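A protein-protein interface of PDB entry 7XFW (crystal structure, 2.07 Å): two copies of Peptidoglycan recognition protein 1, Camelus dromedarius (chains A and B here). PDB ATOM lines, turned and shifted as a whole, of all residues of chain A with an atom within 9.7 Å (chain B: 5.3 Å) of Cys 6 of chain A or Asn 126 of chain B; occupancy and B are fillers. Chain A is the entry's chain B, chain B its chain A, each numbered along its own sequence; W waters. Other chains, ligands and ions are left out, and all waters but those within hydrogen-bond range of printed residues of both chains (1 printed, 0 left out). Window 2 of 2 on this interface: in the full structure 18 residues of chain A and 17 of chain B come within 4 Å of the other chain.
Gly 7 of chain A touches Asn 126 of chain B, and with the chains exchanged Asn 126 of chain A touches Gly 7 of chain B.
Ser 8 of chain A touches Ala 123 of chain B, and with the chains exchanged Ala 123 of chain A touches Ser 8 of chain B.
Ser 8 of chain A touches Asn 126 of chain B, and with the chains exchanged Asn 126 of chain A touches Ser 8 of chain B.
Asn 126 of chain A touches its own counterpart, Asn 126 of chain B.
11 positions are printed for both chains.
Of the 12 pairs that touch across the chains among the printed residues, 9 have their exchanged pair printed and touching as well.
The backbone carbonyl oxygen (O) of Val 81 of chain A lies within hydrogen-bond range of the backbone NH (N) of Val 10 of chain A.
The backbone NH (N) of Gly 7 of chain A sits at hydrogen-bond distance from the side-chain sulfur (SG) of Cys 130 of chain A (3.6 Å).
The side-chain sulfur of Cys 130 of chain A is disulfide-bonded to the side-chain sulfur of Cys 6 of chain A, at 2.1 Å.
The side-chain sulfur (SG) of Cys 130 of chain B lies within hydrogen-bond range of the backbone NH (N) of Gly 7 of chain B (3.1 Å).
Water W1 lies within hydrogen-bond range of O of Ser 8 of chain A (2.8 Å) and NE of Arg 122 of chain B (3.2 Å).
The guanidinium group of Arg 122 of chain B is in hydrogen-bond range of the backbone carbonyl oxygen of Ile 9 of chain A (3.3 Å).
The side-chain hydroxyl of Ser 8 of chain B sits at hydrogen-bond distance from the side-chain amide nitrogen of Asn 126 of chain A, at 2.8 Å.
The side-chain amide oxygen of Asn 126 of chain B lies close to the backbone carbonyl oxygen of Cys 6 of chain A, 3.3 Å away.
Of the printed residues of chain B, Val 10 of chain A touches Arg 122 (3.8 Å).
Of the printed residues of chain B, Arg 122 of chain A touches Ser 8.
Leu 127 of chain A touches none of the printed residues of chain B.
Leu 128 of chain A touches none of the printed residues of chain B.
Printed residues of chain A within 4 Å of Ala 123 of chain B: Ser 8 (3.6 Å).
Asn 126 of chain B touches four residues of chain A.
No residue of chain A comes within 4 Å of Ala 129 of chain B.
The nearest printed residue of chain B that does not touch Cys 6 of chain A is Cys 130 of chain B (5.7 Å).
Among the printed residues, pairs that only touch across the chains: Asn 126 of chain A with Gly 7 of chain B, Arg 122 of chain A with Ser 8 of chain B, Ser 8 of chain A with Asn 126 of chain B, Ser 8 of chain A with Ala 123 of chain B, Gly 7 of chain A with Asn 126 of chain B, Ser 8 of chain A with Arg 122 of chain B, Ala 123 of chain A with Ser 8 of chain B, Val 10 of chain A with Arg 122 of chain B and Asn 126 of chain A with Asn 126 of chain B.
Printed residues of chain B that touch a printed residue of chain A: Gly 7, Ser 8, Arg 122, Ala 123 and Asn 126.
Among the printed residues, no Asp or Glu carboxylate lies within 4 Å of a Lys or Arg side-chain nitrogen of the other chain.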
ATOM      1  N   CYS A   6      20.304 -21.093   5.315  1.00  0.00           N
ATOM      2  CA  CYS A   6      19.017 -20.833   4.614  1.00  0.00           C
ATOM      3  C   CYS A   6      17.828 -20.912   5.569  1.00  0.00           C
ATOM      4  O   CYS A   6      16.894 -20.087   5.431  1.00  0.00           O
ATOM      5  CB  CYS A   6      18.717 -21.864   3.540  1.00  0.00           C
ATOM      6  SG  CYS A   6      17.027 -21.683   2.910  1.00  0.00           S
ATOM      7  N   GLY A   7      17.807 -21.958   6.400  1.00  0.00           N
ATOM      8  CA  GLY A   7      16.814 -22.161   7.470  1.00  0.00           C
ATOM      9  C   GLY A   7      17.498 -22.554   8.767  1.00  0.00           C
ATOM     10  O   GLY A   7      16.873 -23.310   9.556  1.00  0.00           O
ATOM     11  N   SER A   8      18.741 -22.082   8.967  1.00  0.00           N
ATOM     12  CA  SER A   8      19.573 -22.355  10.168  1.00  0.00           C
ATOM     13  C   SER A   8      19.474 -23.845  10.522  1.00  0.00           C
ATOM     14  O   SER A   8      19.042 -24.198  11.656  1.00  0.00           O
ATOM     15  CB  SER A   8      19.156 -21.475  11.307  1.00  0.00           C
ATOM     16  OG  SER A   8      19.694 -20.174  11.138  1.00  0.00           O
ATOM     17  N   ILE A   9      19.840 -24.685   9.561  1.00  0.00           N
ATOM     18  CA  ILE A   9      19.817 -26.167   9.711  1.00  0.00           C
ATOM     19  C   ILE A   9      21.152 -26.582  10.339  1.00  0.00           C
ATOM     20  O   ILE A   9      22.205 -26.201   9.797  1.00  0.00           O
ATOM     21  CB  ILE A   9      19.540 -26.846   8.358  1.00  0.00           C
ATOM     22  CG1 ILE A   9      18.290 -26.267   7.687  1.00  0.00           C
ATOM     23  CG2 ILE A   9      19.430 -28.351   8.522  1.00  0.00           C
ATOM     24  CD1 ILE A   9      18.143 -26.626   6.232  1.00  0.00           C
ATOM     25  N   VAL A  10      21.099 -27.257  11.488  1.00  0.00           N
ATOM     26  CA  VAL A  10      22.252 -27.997  12.075  1.00  0.00           C
ATOM     27  C   VAL A  10      22.666 -29.061  11.058  1.00  0.00           C
ATOM     28  O   VAL A  10      21.858 -29.912  10.667  1.00  0.00           O
ATOM     29  CB  VAL A  10      21.895 -28.596  13.442  1.00  0.00           C
ATOM     30  CG1 VAL A  10      23.116 -29.232  14.085  1.00  0.00           C
ATOM     31  CG2 VAL A  10      21.273 -27.561  14.380  1.00  0.00           C
ATOM     32  N   PHE A  73      14.123 -34.183   7.722  1.00  0.00           N
ATOM     33  CA  PHE A  73      14.581 -33.216   8.754  1.00  0.00           C
ATOM     34  C   PHE A  73      13.934 -33.538  10.088  1.00  0.00           C
ATOM     35  O   PHE A  73      12.805 -34.106  10.077  1.00  0.00           O
ATOM     36  CB  PHE A  73      14.200 -31.787   8.353  1.00  0.00           C
ATOM     37  CG  PHE A  73      14.772 -31.337   7.036  1.00  0.00           C
ATOM     38  CD1 PHE A  73      16.036 -30.761   6.978  1.00  0.00           C
ATOM     39  CD2 PHE A  73      14.065 -31.514   5.864  1.00  0.00           C
ATOM     40  CE1 PHE A  73      16.574 -30.362   5.760  1.00  0.00           C
ATOM     41  CE2 PHE A  73      14.601 -31.115   4.650  1.00  0.00           C
ATOM     42  CZ  PHE A  73      15.841 -30.520   4.601  1.00  0.00           C
ATOM     43  N   GLY A  79      14.306 -25.332  19.132  1.00  0.00           N
ATOM     44  CA  GLY A  79      13.886 -24.405  18.067  1.00  0.00           C
ATOM     45  C   GLY A  79      14.831 -24.410  16.876  1.00  0.00           C
ATOM     46  O   GLY A  79      14.766 -23.466  16.079  1.00  0.00           O
ATOM     47  N   LEU A  80      15.667 -25.445  16.758  1.00  0.00           N
ATOM     48  CA  LEU A  80      16.567 -25.696  15.593  1.00  0.00           C
ATOM     49  C   LEU A  80      16.065 -26.879  14.773  1.00  0.00           C
ATOM     50  O   LEU A  80      15.542 -27.847  15.359  1.00  0.00           O
ATOM     51  CB  LEU A  80      17.984 -26.004  16.089  1.00  0.00           C
ATOM     52  CG  LEU A  80      18.584 -24.989  17.060  1.00  0.00           C
ATOM     53  CD1 LEU A  80      20.022 -25.367  17.372  1.00  0.00           C
ATOM     54  CD2 LEU A  80      18.495 -23.585  16.497  1.00  0.00           C
ATOM     55  N   VAL A  81      16.293 -26.800  13.469  1.00  0.00           N
ATOM     56  CA  VAL A  81      16.101 -27.912  12.510  1.00  0.00           C
ATOM     57  C   VAL A  81      17.407 -28.692  12.423  1.00  0.00           C
ATOM     58  O   VAL A  81      18.476 -28.045  12.425  1.00  0.00           O
ATOM     59  CB  VAL A  81      15.650 -27.376  11.151  1.00  0.00           C
ATOM     60  CG1 VAL A  81      15.321 -28.496  10.208  1.00  0.00           C
ATOM     61  CG2 VAL A  81      14.463 -26.445  11.304  1.00  0.00           C
ATOM     62  N   TRP A  87      16.965 -32.484   1.410  1.00  0.00           N
ATOM     63  CA  TRP A  87      15.945 -32.072   0.393  1.00  0.00           C
ATOM     64  C   TRP A  87      15.879 -33.071  -0.761  1.00  0.00           C
ATOM     65  O   TRP A  87      14.854 -33.111  -1.458  1.00  0.00           O
ATOM     66  CB  TRP A  87      16.222 -30.657  -0.162  1.00  0.00           C
ATOM     67  CG  TRP A  87      15.905 -29.572   0.819  1.00  0.00           C
ATOM     68  CD1 TRP A  87      16.782 -28.722   1.432  1.00  0.00           C
ATOM     69  CD2 TRP A  87      14.612 -29.277   1.375  1.00  0.00           C
ATOM     70  NE1 TRP A  87      16.122 -27.928   2.337  1.00  0.00           N
ATOM     71  CE2 TRP A  87      14.786 -28.240   2.310  1.00  0.00           C
ATOM     72  CE3 TRP A  87      13.328 -29.798   1.182  1.00  0.00           C
ATOM     73  CZ2 TRP A  87      13.723 -27.711   3.041  1.00  0.00           C
ATOM     74  CZ3 TRP A  87      12.281 -29.265   1.898  1.00  0.00           C
ATOM     75  CH2 TRP A  87      12.476 -28.236   2.812  1.00  0.00           C
ATOM     76  N   ARG A 122       7.971 -22.474  14.740  1.00  0.00           N
ATOM     77  CA  ARG A 122       8.598 -21.472  13.819  1.00  0.00           C
ATOM     78  C   ARG A 122       9.666 -22.149  12.947  1.00  0.00           C
ATOM     79  O   ARG A 122       9.702 -21.907  11.745  1.00  0.00           O
ATOM     80  CB  ARG A 122       9.295 -20.337  14.582  1.00  0.00           C
ATOM     81  CG  ARG A 122       8.382 -19.205  15.016  1.00  0.00           C
ATOM     82  CD  ARG A 122       9.190 -17.969  15.373  1.00  0.00           C
ATOM     83  NE  ARG A 122      10.071 -18.214  16.508  1.00  0.00           N
ATOM     84  CZ  ARG A 122       9.694 -18.230  17.783  1.00  0.00           C
ATOM     85  NH1 ARG A 122      10.574 -18.453  18.749  1.00  0.00           N
ATOM     86  NH2 ARG A 122       8.444 -18.012  18.099  1.00  0.00           N
ATOM     87  N   ALA A 123      10.536 -22.951  13.557  1.00  0.00           N
ATOM     88  CA  ALA A 123      11.658 -23.622  12.856  1.00  0.00           C
ATOM     89  C   ALA A 123      11.101 -24.425  11.670  1.00  0.00           C
ATOM     90  O   ALA A 123      11.653 -24.312  10.550  1.00  0.00           O
ATOM     91  CB  ALA A 123      12.403 -24.492  13.836  1.00  0.00           C
ATOM     92  N   GLN A 125       8.086 -24.056  10.118  1.00  0.00           N
ATOM     93  CA  GLN A 125       7.484 -23.147   9.099  1.00  0.00           C
ATOM     94  C   GLN A 125       8.622 -22.480   8.303  1.00  0.00           C
ATOM     95  O   GLN A 125       8.550 -22.433   7.063  1.00  0.00           O
ATOM     96  CB  GLN A 125       6.561 -22.127   9.771  1.00  0.00           C
ATOM     97  CG  GLN A 125       5.406 -22.745  10.544  1.00  0.00           C
ATOM     98  CD  GLN A 125       4.193 -22.996   9.685  1.00  0.00           C
ATOM     99  OE1 GLN A 125       4.287 -23.334   8.506  1.00  0.00           O
ATOM    100  NE2 GLN A 125       3.032 -22.837  10.292  1.00  0.00           N
ATOM    101  N   ASN A 126       9.662 -22.013   8.994  1.00  0.00           N
ATOM    102  CA  ASN A 126      10.883 -21.441   8.355  1.00  0.00           C
ATOM    103  C   ASN A 126      11.476 -22.503   7.418  1.00  0.00           C
ATOM    104  O   ASN A 126      11.662 -22.215   6.204  1.00  0.00           O
ATOM    105  CB  ASN A 126      11.865 -20.935   9.420  1.00  0.00           C
ATOM    106  CG  ASN A 126      13.155 -20.385   8.847  1.00  0.00           C
ATOM    107  OD1 ASN A 126      13.330 -20.335   7.629  1.00  0.00           O
ATOM    108  ND2 ASN A 126      14.073 -19.986   9.718  1.00  0.00           N
ATOM    109  N   LEU A 127      11.701 -23.722   7.926  1.00  0.00           N
ATOM    110  CA  LEU A 127      12.300 -24.809   7.104  1.00  0.00           C
ATOM    111  C   LEU A 127      11.553 -24.927   5.773  1.00  0.00           C
ATOM    112  O   LEU A 127      12.224 -24.999   4.739  1.00  0.00           O
ATOM    113  CB  LEU A 127      12.255 -26.145   7.846  1.00  0.00           C
ATOM    114  CG  LEU A 127      12.698 -27.335   6.998  1.00  0.00           C
ATOM    115  CD1 LEU A 127      14.166 -27.179   6.610  1.00  0.00           C
ATOM    116  CD2 LEU A 127      12.435 -28.662   7.720  1.00  0.00           C
ATOM    117  N   LEU A 128      10.225 -25.005   5.814  1.00  0.00           N
ATOM    118  CA  LEU A 128       9.380 -25.279   4.615  1.00  0.00           C
ATOM    119  C   LEU A 128       9.473 -24.125   3.614  1.00  0.00           C
ATOM    120  O   LEU A 128       9.482 -24.391   2.390  1.00  0.00           O
ATOM    121  CB  LEU A 128       7.925 -25.478   5.042  1.00  0.00           C
ATOM    122  CG  LEU A 128       7.635 -26.734   5.862  1.00  0.00           C
ATOM    123  CD1 LEU A 128       6.129 -26.981   5.937  1.00  0.00           C
ATOM    124  CD2 LEU A 128       8.361 -27.954   5.292  1.00  0.00           C
ATOM    125  N   ALA A 129       9.489 -22.896   4.120  1.00  0.00           N
ATOM    126  CA  ALA A 129       9.652 -21.674   3.300  1.00  0.00           C
ATOM    127  C   ALA A 129      11.024 -21.738   2.606  1.00  0.00           C
ATOM    128  O   ALA A 129      11.065 -21.637   1.361  1.00  0.00           O
ATOM    129  CB  ALA A 129       9.482 -20.450   4.166  1.00  0.00           C
ATOM    130  N   CYS A 130      12.082 -21.995   3.385  1.00  0.00           N
ATOM    131  CA  CYS A 130      13.474 -22.244   2.912  1.00  0.00           C
ATOM    132  C   CYS A 130      13.459 -23.340   1.842  1.00  0.00           C
ATOM    133  O   CYS A 130      14.211 -23.224   0.849  1.00  0.00           O
ATOM    134  CB  CYS A 130      14.394 -22.616   4.074  1.00  0.00           C
ATOM    135  SG  CYS A 130      15.975 -23.344   3.564  1.00  0.00           S
ATOM    136  N   GLY A 131      12.638 -24.377   2.040  1.00  0.00           N
ATOM    137  CA  GLY A 131      12.420 -25.431   1.035  1.00  0.00           C
ATOM    138  C   GLY A 131      11.985 -24.817  -0.276  1.00  0.00           C
ATOM    139  O   GLY A 131      12.688 -25.006  -1.272  1.00  0.00           O
ATOM    140  N   VAL A 132      10.866 -24.082  -0.259  1.00  0.00           N
ATOM    141  CA  VAL A 132      10.280 -23.414  -1.468  1.00  0.00           C
ATOM    142  C   VAL A 132      11.359 -22.490  -2.052  1.00  0.00           C
ATOM    143  O   VAL A 132      11.691 -22.633  -3.250  1.00  0.00           O
ATOM    144  CB  VAL A 132       8.990 -22.624  -1.153  1.00  0.00           C
ATOM    145  CG1 VAL A 132       8.404 -21.997  -2.407  1.00  0.00           C
ATOM    146  CG2 VAL A 132       7.930 -23.468  -0.452  1.00  0.00           C
ATOM    147  N   ALA A 133      11.919 -21.633  -1.191  1.00  0.00           N
ATOM    148  CA  ALA A 133      12.971 -20.639  -1.517  1.00  0.00           C
ATOM    149  C   ALA A 133      14.052 -21.296  -2.378  1.00  0.00           C
ATOM    150  O   ALA A 133      14.327 -20.759  -3.451  1.00  0.00           O
ATOM    151  CB  ALA A 133      13.547 -20.022  -0.262  1.00  0.00           C
ATOM    152  N   LEU A 134      14.623 -22.432  -1.967  1.00  0.00           N
ATOM    153  CA  LEU A 134      15.720 -23.056  -2.758  1.00  0.00           C
ATOM    154  C   LEU A 134      15.155 -24.025  -3.808  1.00  0.00           C
ATOM    155  O   LEU A 134      15.971 -24.593  -4.531  1.00  0.00           O
ATOM    156  CB  LEU A 134      16.768 -23.690  -1.831  1.00  0.00           C
ATOM    157  CG  LEU A 134      16.388 -24.972  -1.100  1.00  0.00           C
ATOM    158  CD1 LEU A 134      16.859 -26.188  -1.864  1.00  0.00           C
ATOM    159  CD2 LEU A 134      16.982 -24.986   0.300  1.00  0.00           C
ATOM    160  N   GLY A 135      13.832 -24.162  -3.950  1.00  0.00           N
ATOM    161  CA  GLY A 135      13.218 -24.926  -5.065  1.00  0.00           C
ATOM    162  C   GLY A 135      13.010 -26.412  -4.777  1.00  0.00           C
ATOM    163  O   GLY A 135      12.626 -27.157  -5.721  1.00  0.00           O
ATOM    164  N   ALA A 136      13.221 -26.839  -3.524  1.00  0.00           N
ATOM    165  CA  ALA A 136      13.076 -28.248  -3.073  1.00  0.00           C
ATOM    166  C   ALA A 136      11.588 -28.600  -2.935  1.00  0.00           C
ATOM    167  O   ALA A 136      11.203 -29.706  -3.348  1.00  0.00           O
ATOM    168  CB  ALA A 136      13.816 -28.459  -1.774  1.00  0.00           C
ATOM    169  N   GLY B   7      12.540 -16.322   7.738  1.00  0.00           N
ATOM    170  CA  GLY B   7      13.456 -16.789   8.798  1.00  0.00           C
ATOM    171  C   GLY B   7      12.753 -16.918  10.136  1.00  0.00           C
ATOM    172  O   GLY B   7      11.589 -16.492  10.237  1.00  0.00           O
ATOM    173  N   SER B   8      13.430 -17.497  11.127  1.00  0.00           N
ATOM    174  CA  SER B   8      12.919 -17.672  12.508  1.00  0.00           C
ATOM    175  C   SER B   8      13.566 -16.610  13.395  1.00  0.00           C
ATOM    176  O   SER B   8      14.797 -16.424  13.302  1.00  0.00           O
ATOM    177  CB  SER B   8      13.177 -19.058  13.029  1.00  0.00           C
ATOM    178  OG  SER B   8      12.628 -20.028  12.152  1.00  0.00           O
ATOM    179  N   LEU B 121      26.533 -18.334  14.390  1.00  0.00           N
ATOM    180  CA  LEU B 121      27.063 -17.702  13.156  1.00  0.00           C
ATOM    181  C   LEU B 121      26.066 -17.893  12.018  1.00  0.00           C
ATOM    182  O   LEU B 121      25.883 -16.927  11.243  1.00  0.00           O
ATOM    183  CB  LEU B 121      28.449 -18.280  12.843  1.00  0.00           C
ATOM    184  CG  LEU B 121      29.551 -17.787  13.788  1.00  0.00           C
ATOM    185  CD1 LEU B 121      30.865 -18.544  13.605  1.00  0.00           C
ATOM    186  CD2 LEU B 121      29.786 -16.302  13.578  1.00  0.00           C
ATOM    187  N   ARG B 122      25.479 -19.092  11.906  1.00  0.00           N
ATOM    188  CA  ARG B 122      24.411 -19.412  10.909  1.00  0.00           C
ATOM    189  C   ARG B 122      23.160 -18.559  11.160  1.00  0.00           C
ATOM    190  O   ARG B 122      22.635 -18.006  10.216  1.00  0.00           O
ATOM    191  CB  ARG B 122      23.947 -20.868  11.005  1.00  0.00           C
ATOM    192  CG  ARG B 122      24.896 -21.903  10.415  1.00  0.00           C
ATOM    193  CD  ARG B 122      24.199 -23.269  10.277  1.00  0.00           C
ATOM    194  NE  ARG B 122      23.837 -23.885  11.541  1.00  0.00           N
ATOM    195  CZ  ARG B 122      24.679 -24.568  12.320  1.00  0.00           C
ATOM    196  NH1 ARG B 122      24.257 -25.088  13.464  1.00  0.00           N
ATOM    197  NH2 ARG B 122      25.943 -24.726  11.967  1.00  0.00           N
ATOM    198  N   ALA B 123      22.702 -18.462  12.406  1.00  0.00           N
ATOM    199  CA  ALA B 123      21.551 -17.604  12.783  1.00  0.00           C
ATOM    200  C   ALA B 123      21.773 -16.186  12.240  1.00  0.00           C
ATOM    201  O   ALA B 123      20.864 -15.638  11.594  1.00  0.00           O
ATOM    202  CB  ALA B 123      21.361 -17.619  14.278  1.00  0.00           C
ATOM    203  N   ALA B 124      22.968 -15.628  12.452  1.00  0.00           N
ATOM    204  CA  ALA B 124      23.339 -14.255  12.037  1.00  0.00           C
ATOM    205  C   ALA B 124      23.260 -14.141  10.508  1.00  0.00           C
ATOM    206  O   ALA B 124      22.622 -13.214  10.026  1.00  0.00           O
ATOM    207  CB  ALA B 124      24.710 -13.889  12.562  1.00  0.00           C
ATOM    208  N   GLN B 125      23.897 -15.045   9.767  1.00  0.00           N
ATOM    209  CA  GLN B 125      23.974 -14.930   8.288  1.00  0.00           C
ATOM    210  C   GLN B 125      22.564 -15.100   7.690  1.00  0.00           C
ATOM    211  O   GLN B 125      22.231 -14.331   6.757  1.00  0.00           O
ATOM    212  CB  GLN B 125      25.036 -15.886   7.745  1.00  0.00           C
ATOM    213  CG  GLN B 125      26.379 -15.660   8.424  1.00  0.00           C
ATOM    214  CD  GLN B 125      27.579 -16.041   7.601  1.00  0.00           C
ATOM    215  OE1 GLN B 125      28.249 -17.032   7.881  1.00  0.00           O
ATOM    216  NE2 GLN B 125      27.879 -15.228   6.601  1.00  0.00           N
ATOM    217  N   ASN B 126      21.763 -16.026   8.221  1.00  0.00           N
ATOM    218  CA  ASN B 126      20.368 -16.293   7.760  1.00  0.00           C
ATOM    219  C   ASN B 126      19.532 -15.022   7.965  1.00  0.00           C
ATOM    220  O   ASN B 126      18.896 -14.563   7.013  1.00  0.00           O
ATOM    221  CB  ASN B 126      19.743 -17.496   8.470  1.00  0.00           C
ATOM    222  CG  ASN B 126      18.368 -17.863   7.942  1.00  0.00           C
ATOM    223  OD1 ASN B 126      17.922 -17.347   6.912  1.00  0.00           O
ATOM    224  ND2 ASN B 126      17.681 -18.753   8.643  1.00  0.00           N
ATOM    225  N   LEU B 127      19.585 -14.442   9.159  1.00  0.00           N
ATOM    226  CA  LEU B 127      18.874 -13.170   9.481  1.00  0.00           C
ATOM    227  C   LEU B 127      19.156 -12.164   8.366  1.00  0.00           C
ATOM    228  O   LEU B 127      18.191 -11.612   7.808  1.00  0.00           O
ATOM    229  CB  LEU B 127      19.330 -12.648  10.849  1.00  0.00           C
ATOM    230  CG  LEU B 127      18.772 -11.275  11.212  1.00  0.00           C
ATOM    231  CD1 LEU B 127      17.294 -11.378  11.570  1.00  0.00           C
ATOM    232  CD2 LEU B 127      19.557 -10.657  12.342  1.00  0.00           C
ATOM    233  N   LEU B 128      20.424 -11.997   7.982  1.00  0.00           N
ATOM    234  CA  LEU B 128      20.806 -10.958   6.988  1.00  0.00           C
ATOM    235  C   LEU B 128      20.163 -11.276   5.628  1.00  0.00           C
ATOM    236  O   LEU B 128      19.691 -10.326   4.971  1.00  0.00           O
ATOM    237  CB  LEU B 128      22.332 -10.810   6.891  1.00  0.00           C
ATOM    238  CG  LEU B 128      23.055 -10.427   8.185  1.00  0.00           C
ATOM    239  CD1 LEU B 128      24.477  -9.990   7.891  1.00  0.00           C
ATOM    240  CD2 LEU B 128      22.328  -9.337   8.961  1.00  0.00           C
ATOM    241  N   ALA B 129      20.137 -12.552   5.230  1.00  0.00           N
ATOM    242  CA  ALA B 129      19.522 -13.006   3.956  1.00  0.00           C
ATOM    243  C   ALA B 129      18.031 -12.651   3.977  1.00  0.00           C
ATOM    244  O   ALA B 129      17.514 -12.164   2.948  1.00  0.00           O
ATOM    245  CB  ALA B 129      19.741 -14.487   3.770  1.00  0.00           C
ATOM    246  N   CYS B 130      17.374 -12.864   5.123  1.00  0.00           N
ATOM    247  CA  CYS B 130      15.945 -12.519   5.340  1.00  0.00           C
ATOM    248  C   CYS B 130      15.753 -11.006   5.260  1.00  0.00           C
ATOM    249  O   CYS B 130      14.757 -10.595   4.665  1.00  0.00           O
ATOM    250  CB  CYS B 130      15.414 -13.081   6.647  1.00  0.00           C
ATOM    251  SG  CYS B 130      14.976 -14.832   6.487  1.00  0.00           S
ATOM    252  N   GLY B 131      16.691 -10.209   5.780  1.00  0.00           N
ATOM    253  CA  GLY B 131      16.655  -8.746   5.606  1.00  0.00           C
ATOM    254  C   GLY B 131      16.683  -8.363   4.140  1.00  0.00           C
ATOM    255  O   GLY B 131      15.921  -7.477   3.734  1.00  0.00           O
HETATM  256  O   HOH W   1      21.228 -23.982  13.324  1.00  0.00           O
